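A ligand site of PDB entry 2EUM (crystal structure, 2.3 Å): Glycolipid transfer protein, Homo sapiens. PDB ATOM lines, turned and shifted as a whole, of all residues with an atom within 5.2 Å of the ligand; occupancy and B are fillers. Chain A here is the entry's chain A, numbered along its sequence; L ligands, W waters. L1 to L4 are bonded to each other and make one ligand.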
ATOM      1  N   PHE A  34     -12.982 -22.727   9.243  1.00  0.00           N
ATOM      2  CA  PHE A  34     -11.674 -23.319   8.933  1.00  0.00           C
ATOM      3  C   PHE A  34     -10.501 -22.636   9.654  1.00  0.00           C
ATOM      4  O   PHE A  34      -9.446 -23.244   9.845  1.00  0.00           O
ATOM      5  CB  PHE A  34     -11.413 -23.372   7.428  1.00  0.00           C
ATOM      6  CG  PHE A  34     -12.179 -24.444   6.724  1.00  0.00           C
ATOM      7  CD1 PHE A  34     -11.749 -25.768   6.782  1.00  0.00           C
ATOM      8  CD2 PHE A  34     -13.335 -24.130   6.013  1.00  0.00           C
ATOM      9  CE1 PHE A  34     -12.462 -26.761   6.136  1.00  0.00           C
ATOM     10  CE2 PHE A  34     -14.056 -25.126   5.362  1.00  0.00           C
ATOM     11  CZ  PHE A  34     -13.614 -26.447   5.416  1.00  0.00           C
ATOM     12  N   PRO A  44      -5.546 -23.244   2.354  1.00  0.00           N
ATOM     13  CA  PRO A  44      -5.866 -23.564   0.950  1.00  0.00           C
ATOM     14  C   PRO A  44      -7.266 -24.156   0.762  1.00  0.00           C
ATOM     15  O   PRO A  44      -7.867 -23.997  -0.299  1.00  0.00           O
ATOM     16  CB  PRO A  44      -4.807 -24.608   0.585  1.00  0.00           C
ATOM     17  CG  PRO A  44      -3.683 -24.351   1.524  1.00  0.00           C
ATOM     18  CD  PRO A  44      -4.373 -24.031   2.806  1.00  0.00           C
ATOM     19  N   ILE A  45      -7.759 -24.841   1.794  1.00  0.00           N
ATOM     20  CA  ILE A  45      -9.075 -25.424   1.780  1.00  0.00           C
ATOM     21  C   ILE A  45     -10.127 -24.330   1.869  1.00  0.00           C
ATOM     22  O   ILE A  45     -11.097 -24.338   1.100  1.00  0.00           O
ATOM     23  CB  ILE A  45      -9.246 -26.415   2.918  1.00  0.00           C
ATOM     24  CG1 ILE A  45      -8.344 -27.646   2.704  1.00  0.00           C
ATOM     25  CG2 ILE A  45     -10.698 -26.810   3.057  1.00  0.00           C
ATOM     26  CD1 ILE A  45      -8.378 -28.662   3.864  1.00  0.00           C
ATOM     27  N   ASP A  48     -10.233 -22.349  -1.480  1.00  0.00           N
ATOM     28  CA  ASP A  48     -10.921 -22.997  -2.566  1.00  0.00           C
ATOM     29  C   ASP A  48     -12.428 -22.818  -2.433  1.00  0.00           C
ATOM     30  O   ASP A  48     -13.124 -22.585  -3.431  1.00  0.00           O
ATOM     31  CB  ASP A  48     -10.576 -24.487  -2.634  1.00  0.00           C
ATOM     32  CG  ASP A  48     -11.272 -25.194  -3.768  1.00  0.00           C
ATOM     33  OD1 ASP A  48     -10.670 -25.330  -4.862  1.00  0.00           O
ATOM     34  OD2 ASP A  48     -12.459 -25.576  -3.579  1.00  0.00           O
ATOM     35  N   ILE A  49     -12.918 -22.924  -1.201  1.00  0.00           N
ATOM     36  CA  ILE A  49     -14.356 -22.795  -0.978  1.00  0.00           C
ATOM     37  C   ILE A  49     -14.779 -21.334  -1.181  1.00  0.00           C
ATOM     38  O   ILE A  49     -15.718 -21.070  -1.930  1.00  0.00           O
ATOM     39  CB  ILE A  49     -14.812 -23.388   0.392  1.00  0.00           C
ATOM     40  CG1 ILE A  49     -14.516 -24.893   0.444  1.00  0.00           C
ATOM     41  CG2 ILE A  49     -16.318 -23.164   0.625  1.00  0.00           C
ATOM     42  CD1 ILE A  49     -14.633 -25.525   1.790  1.00  0.00           C
ATOM     43  N   ASN A  52     -14.639 -20.248  -4.926  1.00  0.00           N
ATOM     44  CA  ASN A  52     -15.787 -20.735  -5.660  1.00  0.00           C
ATOM     45  C   ASN A  52     -17.049 -19.938  -5.366  1.00  0.00           C
ATOM     46  O   ASN A  52     -17.752 -19.556  -6.281  1.00  0.00           O
ATOM     47  CB  ASN A  52     -15.992 -22.217  -5.406  1.00  0.00           C
ATOM     48  CG  ASN A  52     -15.082 -23.052  -6.237  1.00  0.00           C
ATOM     49  OD1 ASN A  52     -14.700 -22.665  -7.349  1.00  0.00           O
ATOM     50  ND2 ASN A  52     -14.699 -24.191  -5.716  1.00  0.00           N
ATOM     51  N   LYS A  55     -16.566 -16.688  -7.157  1.00  0.00           N
ATOM     52  CA  LYS A  55     -16.812 -16.899  -8.605  1.00  0.00           C
ATOM     53  C   LYS A  55     -18.299 -16.882  -8.981  1.00  0.00           C
ATOM     54  O   LYS A  55     -18.704 -16.216  -9.936  1.00  0.00           O
ATOM     55  CB  LYS A  55     -16.160 -18.212  -9.106  1.00  0.00           C
ATOM     56  CG  LYS A  55     -14.742 -18.062  -9.678  1.00  0.00           C
ATOM     57  CD  LYS A  55     -13.756 -19.180  -9.210  1.00  0.00           C
ATOM     58  CE  LYS A  55     -12.270 -18.736  -9.245  1.00  0.00           C
ATOM     59  NZ  LYS A  55     -11.346 -19.625  -8.434  1.00  0.00           N
ATOM     60  N   GLY A  89     -17.383 -21.155 -16.237  1.00  0.00           N
ATOM     61  CA  GLY A  89     -18.225 -20.207 -15.521  1.00  0.00           C
ATOM     62  C   GLY A  89     -18.620 -20.564 -14.104  1.00  0.00           C
ATOM     63  O   GLY A  89     -17.869 -21.213 -13.382  1.00  0.00           O
ATOM     64  N   LEU A  92     -19.047 -24.420 -13.284  1.00  0.00           N
ATOM     65  CA  LEU A  92     -17.842 -25.137 -12.874  1.00  0.00           C
ATOM     66  C   LEU A  92     -17.463 -24.835 -11.419  1.00  0.00           C
ATOM     67  O   LEU A  92     -17.036 -25.727 -10.671  1.00  0.00           O
ATOM     68  CB  LEU A  92     -16.666 -24.856 -13.833  1.00  0.00           C
ATOM     69  CG  LEU A  92     -15.351 -25.549 -13.526  1.00  0.00           C
ATOM     70  CD1 LEU A  92     -15.494 -27.088 -13.441  1.00  0.00           C
ATOM     71  CD2 LEU A  92     -14.326 -25.162 -14.571  1.00  0.00           C
ATOM     72  N   ALA A  93     -17.631 -23.575 -11.027  1.00  0.00           N
ATOM     73  CA  ALA A  93     -17.353 -23.147  -9.657  1.00  0.00           C
ATOM     74  C   ALA A  93     -18.246 -23.899  -8.662  1.00  0.00           C
ATOM     75  O   ALA A  93     -17.758 -24.455  -7.669  1.00  0.00           O
ATOM     76  CB  ALA A  93     -17.511 -21.630  -9.521  1.00  0.00           C
ATOM     77  N   TRP A  96     -17.557 -27.678  -7.926  1.00  0.00           N
ATOM     78  CA  TRP A  96     -16.523 -27.911  -6.920  1.00  0.00           C
ATOM     79  C   TRP A  96     -16.918 -27.409  -5.533  1.00  0.00           C
ATOM     80  O   TRP A  96     -16.505 -27.990  -4.509  1.00  0.00           O
ATOM     81  CB  TRP A  96     -15.200 -27.297  -7.370  1.00  0.00           C
ATOM     82  CG  TRP A  96     -14.500 -28.115  -8.425  1.00  0.00           C
ATOM     83  CD1 TRP A  96     -14.502 -27.901  -9.776  1.00  0.00           C
ATOM     84  CD2 TRP A  96     -13.707 -29.308  -8.216  1.00  0.00           C
ATOM     85  NE1 TRP A  96     -13.757 -28.873 -10.416  1.00  0.00           N
ATOM     86  CE2 TRP A  96     -13.253 -29.734  -9.476  1.00  0.00           C
ATOM     87  CE3 TRP A  96     -13.338 -30.047  -7.077  1.00  0.00           C
ATOM     88  CZ2 TRP A  96     -12.432 -30.863  -9.633  1.00  0.00           C
ATOM     89  CZ3 TRP A  96     -12.533 -31.150  -7.230  1.00  0.00           C
ATOM     90  CH2 TRP A  96     -12.082 -31.558  -8.504  1.00  0.00           C
ATOM     91  N   GLY A 100     -17.126 -29.572  -1.809  1.00  0.00           N
ATOM     92  CA  GLY A 100     -16.599 -29.070  -0.531  1.00  0.00           C
ATOM     93  C   GLY A 100     -17.703 -28.980   0.510  1.00  0.00           C
ATOM     94  O   GLY A 100     -17.492 -29.246   1.685  1.00  0.00           O
ATOM     95  N   PHE A 103     -18.624 -32.457   1.483  1.00  0.00           N
ATOM     96  CA  PHE A 103     -17.604 -32.891   2.408  1.00  0.00           C
ATOM     97  C   PHE A 103     -17.953 -32.453   3.819  1.00  0.00           C
ATOM     98  O   PHE A 103     -17.893 -33.250   4.743  1.00  0.00           O
ATOM     99  CB  PHE A 103     -16.213 -32.412   2.016  1.00  0.00           C
ATOM    100  CG  PHE A 103     -15.157 -32.784   3.002  1.00  0.00           C
ATOM    101  CD1 PHE A 103     -14.388 -33.922   2.810  1.00  0.00           C
ATOM    102  CD2 PHE A 103     -14.972 -32.029   4.176  1.00  0.00           C
ATOM    103  CE1 PHE A 103     -13.432 -34.292   3.747  1.00  0.00           C
ATOM    104  CE2 PHE A 103     -14.029 -32.404   5.119  1.00  0.00           C
ATOM    105  CZ  PHE A 103     -13.247 -33.542   4.899  1.00  0.00           C
ATOM    106  N   LEU A 136     -14.913 -36.131  -2.187  1.00  0.00           N
ATOM    107  CA  LEU A 136     -13.790 -35.569  -2.933  1.00  0.00           C
ATOM    108  C   LEU A 136     -12.828 -36.564  -3.591  1.00  0.00           C
ATOM    109  O   LEU A 136     -12.307 -36.273  -4.656  1.00  0.00           O
ATOM    110  CB  LEU A 136     -12.984 -34.625  -2.040  1.00  0.00           C
ATOM    111  CG  LEU A 136     -13.616 -33.305  -1.641  1.00  0.00           C
ATOM    112  CD1 LEU A 136     -12.778 -32.678  -0.537  1.00  0.00           C
ATOM    113  CD2 LEU A 136     -13.709 -32.385  -2.840  1.00  0.00           C
ATOM    114  N   HIS A 140      -9.652 -36.650  -7.174  1.00  0.00           N
ATOM    115  CA  HIS A 140      -8.256 -36.353  -6.904  1.00  0.00           C
ATOM    116  C   HIS A 140      -7.336 -37.431  -7.458  1.00  0.00           C
ATOM    117  O   HIS A 140      -7.546 -38.618  -7.212  1.00  0.00           O
ATOM    118  CB  HIS A 140      -8.008 -36.151  -5.399  1.00  0.00           C
ATOM    119  CG  HIS A 140      -8.701 -34.953  -4.838  1.00  0.00           C
ATOM    120  ND1 HIS A 140      -8.923 -34.795  -3.482  1.00  0.00           N
ATOM    121  CD2 HIS A 140      -9.242 -33.864  -5.434  1.00  0.00           C
ATOM    122  CE1 HIS A 140      -9.553 -33.651  -3.278  1.00  0.00           C
ATOM    123  NE2 HIS A 140      -9.761 -33.072  -4.447  1.00  0.00           N
ATOM    124  N   VAL A 144      -2.687 -35.398  -4.783  1.00  0.00           N
ATOM    125  CA  VAL A 144      -3.583 -34.639  -3.921  1.00  0.00           C
ATOM    126  C   VAL A 144      -4.119 -35.533  -2.795  1.00  0.00           C
ATOM    127  O   VAL A 144      -4.316 -35.083  -1.666  1.00  0.00           O
ATOM    128  CB  VAL A 144      -4.740 -34.017  -4.740  1.00  0.00           C
ATOM    129  CG1 VAL A 144      -5.740 -33.283  -3.839  1.00  0.00           C
ATOM    130  CG2 VAL A 144      -4.200 -33.074  -5.799  1.00  0.00           C
ATOM    131  N   ILE A 147      -1.532 -35.812  -0.247  1.00  0.00           N
ATOM    132  CA  ILE A 147      -1.591 -34.542   0.475  1.00  0.00           C
ATOM    133  C   ILE A 147      -2.725 -34.478   1.503  1.00  0.00           C
ATOM    134  O   ILE A 147      -2.483 -34.123   2.668  1.00  0.00           O
ATOM    135  CB  ILE A 147      -1.588 -33.312  -0.472  1.00  0.00           C
ATOM    136  CG1 ILE A 147      -0.255 -33.229  -1.228  1.00  0.00           C
ATOM    137  CG2 ILE A 147      -1.881 -32.013   0.325  1.00  0.00           C
ATOM    138  CD1 ILE A 147      -0.263 -32.334  -2.451  1.00  0.00           C
ATOM    139  N   TYR A 207     -13.350 -35.474 -14.113  1.00  0.00           N
ATOM    140  CA  TYR A 207     -11.916 -35.298 -14.256  1.00  0.00           C
ATOM    141  C   TYR A 207     -11.255 -35.142 -12.895  1.00  0.00           C
ATOM    142  O   TYR A 207     -11.835 -34.556 -11.965  1.00  0.00           O
ATOM    143  CB  TYR A 207     -11.595 -34.129 -15.181  1.00  0.00           C
ATOM    144  CG  TYR A 207     -11.824 -32.762 -14.598  1.00  0.00           C
ATOM    145  CD1 TYR A 207     -10.807 -32.081 -13.932  1.00  0.00           C
ATOM    146  CD2 TYR A 207     -13.055 -32.127 -14.731  1.00  0.00           C
ATOM    147  CE1 TYR A 207     -11.015 -30.809 -13.415  1.00  0.00           C
ATOM    148  CE2 TYR A 207     -13.280 -30.864 -14.222  1.00  0.00           C
ATOM    149  CZ  TYR A 207     -12.260 -30.205 -13.564  1.00  0.00           C
ATOM    150  OH  TYR A 207     -12.488 -28.956 -13.056  1.00  0.00           O
ATOM    151  N   VAL A 209      -7.907 -34.106 -10.372  1.00  0.00           N
ATOM    152  CA  VAL A 209      -6.885 -33.054 -10.289  1.00  0.00           C
ATOM    153  C   VAL A 209      -5.578 -33.530  -9.690  1.00  0.00           C
ATOM    154  O   VAL A 209      -5.526 -34.440  -8.856  1.00  0.00           O
ATOM    155  CB  VAL A 209      -7.391 -31.739  -9.606  1.00  0.00           C
ATOM    156  CG1 VAL A 209      -8.503 -31.091 -10.447  1.00  0.00           C
ATOM    157  CG2 VAL A 209      -7.816 -31.960  -8.173  1.00  0.00           C
ATOM    158  OXT VAL A 209      -4.517 -33.008 -10.054  1.00  0.00           O
HETATM  159  C1  LIG L   1     -12.218 -23.140 -12.426  1.00  0.00           C
HETATM  160  C2  LIG L   1     -12.239 -21.750 -11.788  1.00  0.00           C
HETATM  161  C3  LIG L   1     -11.856 -20.678 -12.815  1.00  0.00           C
HETATM  162  C4  LIG L   1     -10.540 -21.042 -13.503  1.00  0.00           C
HETATM  163  C5  LIG L   1     -10.678 -22.476 -14.040  1.00  0.00           C
HETATM  164  C6  LIG L   1      -9.503 -22.967 -14.883  1.00  0.00           C
HETATM  165  O1  LIG L   1     -13.543 -21.519 -11.314  1.00  0.00           O
HETATM  166  O2  LIG L   1     -11.785 -19.403 -12.218  1.00  0.00           O
HETATM  167  O3  LIG L   1      -9.449 -20.923 -12.622  1.00  0.00           O
HETATM  168  O4  LIG L   1     -10.947 -23.385 -12.995  1.00  0.00           O
HETATM  169  O5  LIG L   1     -10.044 -23.921 -15.780  1.00  0.00           O
HETATM  170  C1  LG2 L   2     -11.488 -25.022  -8.043  1.00  0.00           C
HETATM  171  C2  LG2 L   2     -12.361 -24.517  -9.177  1.00  0.00           C
HETATM  172  C3  LG2 L   2     -11.647 -24.610 -10.530  1.00  0.00           C
HETATM  173  C4  LG2 L   2     -11.279 -26.062 -10.821  1.00  0.00           C
HETATM  174  C5  LG2 L   2     -10.434 -26.201 -12.087  1.00  0.00           C
HETATM  175  C6  LG2 L   2     -10.513 -26.162  -8.436  1.00  0.00           C
HETATM  176  O1  LG2 L   2     -10.573 -27.193  -7.488  1.00  0.00           O
HETATM  177  O2  LG2 L   2     -12.298 -25.381  -6.939  1.00  0.00           O
HETATM  178  O3  LG2 L   2     -12.800 -23.194  -8.929  1.00  0.00           O
HETATM  179  O4  LG2 L   2     -12.551 -24.174 -11.521  1.00  0.00           O
HETATM  180  O5  LG2 L   2     -10.628 -26.727  -9.736  1.00  0.00           O
HETATM  181  O6  LG2 L   2     -10.472 -27.556 -12.510  1.00  0.00           O
HETATM  182  C1  LG3 L   3     -10.021 -28.409  -7.472  1.00  0.00           C
HETATM  183  C2  LG3 L   3      -9.572 -28.857  -6.078  1.00  0.00           C
HETATM  184  N1  LG3 L   3     -10.656 -28.711  -5.117  1.00  0.00           N
HETATM  185  C3  LG3 L   3      -8.328 -28.106  -5.581  1.00  0.00           C
HETATM  186  O1  LG3 L   3      -7.240 -28.368  -6.471  1.00  0.00           O
HETATM  187  C4  LG3 L   3      -7.964 -28.494  -4.151  1.00  0.00           C
HETATM  188  C5  LG3 L   3      -7.711 -27.564  -3.215  1.00  0.00           C
HETATM  189  C6  LG3 L   3      -7.190 -27.951  -1.832  1.00  0.00           C
HETATM  190  C7  LG3 L   3      -5.662 -27.770  -1.685  1.00  0.00           C
HETATM  191  C8  LG3 L   3      -4.868 -28.974  -2.219  1.00  0.00           C
HETATM  192  C9  LG3 L   3      -3.637 -28.554  -3.010  1.00  0.00           C
HETATM  193  C10 LG3 L   3      -2.366 -29.086  -2.350  1.00  0.00           C
HETATM  194  C11 LG3 L   3      -1.165 -28.199  -2.642  1.00  0.00           C
HETATM  195  C12 LG3 L   3      -0.119 -28.315  -1.533  1.00  0.00           C
HETATM  196  C13 LG3 L   3       0.851 -27.124  -1.522  1.00  0.00           C
HETATM  197  C14 LG3 L   3       2.235 -27.510  -2.044  1.00  0.00           C
HETATM  198  C15 LG3 L   3       3.219 -27.875  -0.937  1.00  0.00           C
HETATM  199  C16 LG3 L   3       3.703 -26.656  -0.139  1.00  0.00           C
HETATM  200  C17 LG3 L   3       4.989 -26.946   0.634  1.00  0.00           C
HETATM  201  C18 LG3 L   3       5.629 -25.641   1.083  1.00  0.00           C
HETATM  202  C1  LG4 L   4     -11.622 -29.120  -4.432  1.00  0.00           C
HETATM  203  C2  LG4 L   4     -12.451 -28.856  -3.183  1.00  0.00           C
HETATM  204  C3  LG4 L   4     -11.528 -28.520  -2.009  1.00  0.00           C
HETATM  205  C4  LG4 L   4     -12.344 -28.368  -0.741  1.00  0.00           C
HETATM  206  C5  LG4 L   4     -11.714 -29.154   0.392  1.00  0.00           C
HETATM  207  C6  LG4 L   4     -12.767 -29.522   1.423  1.00  0.00           C
HETATM  208  C7  LG4 L   4     -12.125 -30.407   2.487  1.00  0.00           C
HETATM  209  O1  LG4 L   4     -10.857 -30.326  -4.280  1.00  0.00           O
HETATM  210  O   HOH W   1      -8.413 -22.934 -10.066  1.00  0.00           O
HETATM  211  O   HOH W   2     -15.179 -21.243 -13.301  1.00  0.00           O
HETATM  212  O   HOH W   3     -12.549 -17.251 -13.434  1.00  0.00           O
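An oxygen (O3) of LG2 L2 sits at hydrogen-bond distance from the side-chain amide oxygen (OD1) of Asn 52 (2.5 Å). The side-chain hydroxyl (OH) of Tyr 207 sits at hydrogen-bond distance from an oxygen (O6) of LG2 L2. The side-chain carboxylate of Asp 48 sits at hydrogen-bond distance from an oxygen (O2) of LG2 L2. O1 of LG4 L4 sits at hydrogen-bond distance from NE2 of His 140 (3.0 Å).
The side-chain hydroxyl (OH) of Tyr 207 is in hydrogen-bond range of the indole nitrogen (NE1) of Trp 96 (2.9 Å). The side-chain amide nitrogen (ND2) of Asn 52 sits at hydrogen-bond distance from the backbone carbonyl oxygen (O) of Asp 48 (3.2 Å).
Residues that only touch the ligand: Lys 55, Trp 96, Leu 92, Phe 103, Ile 45, Leu 136, Ile 147 and Pro 44. Hydrophobic or aromatic side chains that line the ligand: Pro 44, Ile 45, Leu 92, Trp 96, Phe 103, Leu 136, His 140, Ile 147 and Tyr 207. Within 4 Å of the ligand: Pro 44, Ile 45, Asp 48, Asn 52, Lys 55, Leu 92, Trp 96, Phe 103, Leu 136, His 140, Ile 147 and Tyr 207. Along chain A the residues within 4 Å of the ligand span positions 44 to 207.
Water W2 bridges O1 of LIG L1 (2.6 Å) and O of Gly 89 (2.7 Å).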
